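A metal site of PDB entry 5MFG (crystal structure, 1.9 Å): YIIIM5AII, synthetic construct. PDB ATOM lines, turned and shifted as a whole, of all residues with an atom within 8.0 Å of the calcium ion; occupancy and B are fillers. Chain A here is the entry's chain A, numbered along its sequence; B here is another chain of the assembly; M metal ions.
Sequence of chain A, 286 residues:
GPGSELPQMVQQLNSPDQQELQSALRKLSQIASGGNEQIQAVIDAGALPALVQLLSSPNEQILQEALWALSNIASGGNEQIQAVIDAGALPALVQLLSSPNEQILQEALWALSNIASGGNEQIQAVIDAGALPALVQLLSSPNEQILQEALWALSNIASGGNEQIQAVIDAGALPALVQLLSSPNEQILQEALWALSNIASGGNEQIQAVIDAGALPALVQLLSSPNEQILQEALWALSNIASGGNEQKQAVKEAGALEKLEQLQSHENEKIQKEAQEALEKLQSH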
ATOM      1  N   SER A  15      -2.749   6.279   4.028  1.00  0.00           N
ATOM      2  CA  SER A  15      -3.758   7.322   4.071  1.00  0.00           C
ATOM      3  C   SER A  15      -3.252   8.490   4.912  1.00  0.00           C
ATOM      4  O   SER A  15      -2.664   8.293   5.977  1.00  0.00           O
ATOM      5  CB  SER A  15      -5.057   6.779   4.662  1.00  0.00           C
ATOM      6  OG  SER A  15      -6.050   7.788   4.719  1.00  0.00           O
ATOM      7  N   PRO A  16      -3.465   9.733   4.455  1.00  0.00           N
ATOM      8  CA  PRO A  16      -3.143  10.884   5.314  1.00  0.00           C
ATOM      9  C   PRO A  16      -4.183  11.130   6.385  1.00  0.00           C
ATOM     10  O   PRO A  16      -3.987  12.018   7.228  1.00  0.00           O
ATOM     11  CB  PRO A  16      -3.079  12.053   4.317  1.00  0.00           C
ATOM     12  CG  PRO A  16      -3.480  11.497   2.976  1.00  0.00           C
ATOM     13  CD  PRO A  16      -4.095  10.160   3.208  1.00  0.00           C
ATOM     14  N   ASP A  17      -5.280  10.383   6.377  1.00  0.00           N
ATOM     15  CA  ASP A  17      -6.328  10.524   7.377  1.00  0.00           C
ATOM     16  C   ASP A  17      -5.935   9.716   8.610  1.00  0.00           C
ATOM     17  O   ASP A  17      -6.022   8.483   8.595  1.00  0.00           O
ATOM     18  CB  ASP A  17      -7.665  10.061   6.798  1.00  0.00           C
ATOM     19  CG  ASP A  17      -8.815  10.248   7.761  1.00  0.00           C
ATOM     20  OD1 ASP A  17      -8.659   9.925   8.951  1.00  0.00           O
ATOM     21  OD2 ASP A  17      -9.875  10.732   7.306  1.00  0.00           O
ATOM     22  N   GLN A  18      -5.497  10.397   9.661  1.00  0.00           N
ATOM     23  CA  GLN A  18      -5.005   9.709  10.851  1.00  0.00           C
ATOM     24  C   GLN A  18      -6.071   8.793  11.444  1.00  0.00           C
ATOM     25  O   GLN A  18      -5.759   7.706  11.957  1.00  0.00           O
ATOM     26  CB  GLN A  18      -4.534  10.715  11.894  1.00  0.00           C
ATOM     27  CG  GLN A  18      -3.186  11.340  11.597  1.00  0.00           C
ATOM     28  CD  GLN A  18      -3.283  12.580  10.738  1.00  0.00           C
ATOM     29  OE1 GLN A  18      -4.283  12.812  10.065  1.00  0.00           O
ATOM     30  NE2 GLN A  18      -2.232  13.393  10.756  1.00  0.00           N
ATOM     31  N   GLN A  19      -7.337   9.209  11.404  1.00  0.00           N
ATOM     32  CA  GLN A  19      -8.404   8.365  11.930  1.00  0.00           C
ATOM     33  C   GLN A  19      -8.556   7.103  11.099  1.00  0.00           C
ATOM     34  O   GLN A  19      -8.753   6.014  11.656  1.00  0.00           O
ATOM     35  CB  GLN A  19      -9.711   9.156  11.969  1.00  0.00           C
ATOM     36  CG  GLN A  19     -10.890   8.398  12.556  1.00  0.00           C
ATOM     37  CD  GLN A  19     -11.732   7.707  11.512  1.00  0.00           C
ATOM     38  OE1 GLN A  19     -11.364   7.638  10.336  1.00  0.00           O
ATOM     39  NE2 GLN A  19     -12.882   7.188  11.921  1.00  0.00           N
ATOM     40  N   SER B 225      -6.871  21.094  14.238  1.00  0.00           N
ATOM     41  CA  SER B 225      -5.838  20.119  13.934  1.00  0.00           C
ATOM     42  C   SER B 225      -6.121  19.461  12.591  1.00  0.00           C
ATOM     43  O   SER B 225      -7.277  19.198  12.253  1.00  0.00           O
ATOM     44  CB  SER B 225      -5.766  19.066  15.032  1.00  0.00           C
ATOM     45  OG  SER B 225      -4.795  18.077  14.723  1.00  0.00           O
ATOM     46  N   PRO B 226      -5.087  19.182  11.788  1.00  0.00           N
ATOM     47  CA  PRO B 226      -5.282  18.372  10.583  1.00  0.00           C
ATOM     48  C   PRO B 226      -5.360  16.878  10.865  1.00  0.00           C
ATOM     49  O   PRO B 226      -5.638  16.105   9.937  1.00  0.00           O
ATOM     50  CB  PRO B 226      -4.042  18.693   9.743  1.00  0.00           C
ATOM     51  CG  PRO B 226      -2.996  19.024  10.739  1.00  0.00           C
ATOM     52  CD  PRO B 226      -3.701  19.691  11.889  1.00  0.00           C
ATOM     53  N   ASN B 227      -5.124  16.463  12.103  1.00  0.00           N
ATOM     54  CA  ASN B 227      -5.146  15.057  12.476  1.00  0.00           C
ATOM     55  C   ASN B 227      -6.595  14.623  12.692  1.00  0.00           C
ATOM     56  O   ASN B 227      -7.237  15.064  13.648  1.00  0.00           O
ATOM     57  CB  ASN B 227      -4.313  14.827  13.721  1.00  0.00           C
ATOM     58  CG  ASN B 227      -4.269  13.367  14.148  1.00  0.00           C
ATOM     59  OD1 ASN B 227      -5.263  12.657  14.050  1.00  0.00           O
ATOM     60  ND2 ASN B 227      -3.117  12.935  14.627  1.00  0.00           N
ATOM     61  N   GLU B 228      -7.094  13.753  11.816  1.00  0.00           N
ATOM     62  CA  GLU B 228      -8.483  13.339  11.906  1.00  0.00           C
ATOM     63  C   GLU B 228      -8.746  12.524  13.174  1.00  0.00           C
ATOM     64  O   GLU B 228      -9.877  12.528  13.684  1.00  0.00           O
ATOM     65  CB  GLU B 228      -8.878  12.531  10.670  1.00  0.00           C
ATOM     66  CG  GLU B 228      -9.028  13.362   9.414  1.00  0.00           C
ATOM     67  CD  GLU B 228      -7.716  13.901   8.915  1.00  0.00           C
ATOM     68  OE1 GLU B 228      -6.676  13.271   9.198  1.00  0.00           O
ATOM     69  OE2 GLU B 228      -7.705  14.957   8.250  1.00  0.00           O
ATOM     70  N   GLN B 229      -7.745  11.817  13.684  1.00  0.00           N
ATOM     71  CA  GLN B 229      -7.926  11.083  14.921  1.00  0.00           C
ATOM     72  C   GLN B 229      -8.059  12.019  16.112  1.00  0.00           C
ATOM     73  O   GLN B 229      -8.851  11.774  17.021  1.00  0.00           O
ATOM     74  CB  GLN B 229      -6.762  10.111  15.145  1.00  0.00           C
ATOM     75  CG  GLN B 229      -6.885   9.266  16.394  1.00  0.00           C
ATOM     76  CD  GLN B 229      -8.091   8.359  16.370  1.00  0.00           C
ATOM     77  OE1 GLN B 229      -8.428   7.772  15.343  1.00  0.00           O
ATOM     78  NE2 GLN B 229      -8.763   8.230  17.522  1.00  0.00           N
ATOM     79  N   LEU B 231      -9.189  15.253  15.965  1.00  0.00           N
ATOM     80  CA  LEU B 231     -10.505  15.852  15.814  1.00  0.00           C
ATOM     81  C   LEU B 231     -11.587  14.927  16.384  1.00  0.00           C
ATOM     82  O   LEU B 231     -12.414  15.340  17.203  1.00  0.00           O
ATOM     83  CB  LEU B 231     -10.775  16.165  14.350  1.00  0.00           C
ATOM     84  CG  LEU B 231      -9.824  17.128  13.637  1.00  0.00           C
ATOM     85  CD1 LEU B 231     -10.136  17.216  12.149  1.00  0.00           C
ATOM     86  CD2 LEU B 231      -9.886  18.516  14.256  1.00  0.00           C
ATOM     87  N   HIS B 267     -16.310  18.208   6.325  1.00  0.00           N
ATOM     88  CA  HIS B 267     -15.033  17.514   6.323  1.00  0.00           C
ATOM     89  C   HIS B 267     -15.117  16.261   5.458  1.00  0.00           C
ATOM     90  O   HIS B 267     -16.167  15.642   5.324  1.00  0.00           O
ATOM     91  CB  HIS B 267     -14.608  17.159   7.747  1.00  0.00           C
ATOM     92  CG  HIS B 267     -13.152  16.880   7.884  1.00  0.00           C
ATOM     93  ND1 HIS B 267     -12.615  15.608   7.864  1.00  0.00           N
ATOM     94  CD2 HIS B 267     -12.097  17.713   8.060  1.00  0.00           C
ATOM     95  CE1 HIS B 267     -11.307  15.670   8.008  1.00  0.00           C
ATOM     96  NE2 HIS B 267     -10.967  16.939   8.126  1.00  0.00           N
HETATM   97 CA    CA M   1      -5.053  14.479   8.262  1.00  0.00          CA
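The calcium ion is bound by OE1 of Glu 228 of chain B (2.2 Å), O of Pro 226 of chain B (2.4 Å), OE1 of Gln 18 (2.6 Å), OE2 of Glu 228 of chain B (2.7 Å) and O of Pro 16 (2.9 Å).
The calcium ion has five donor atoms within binding distance.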
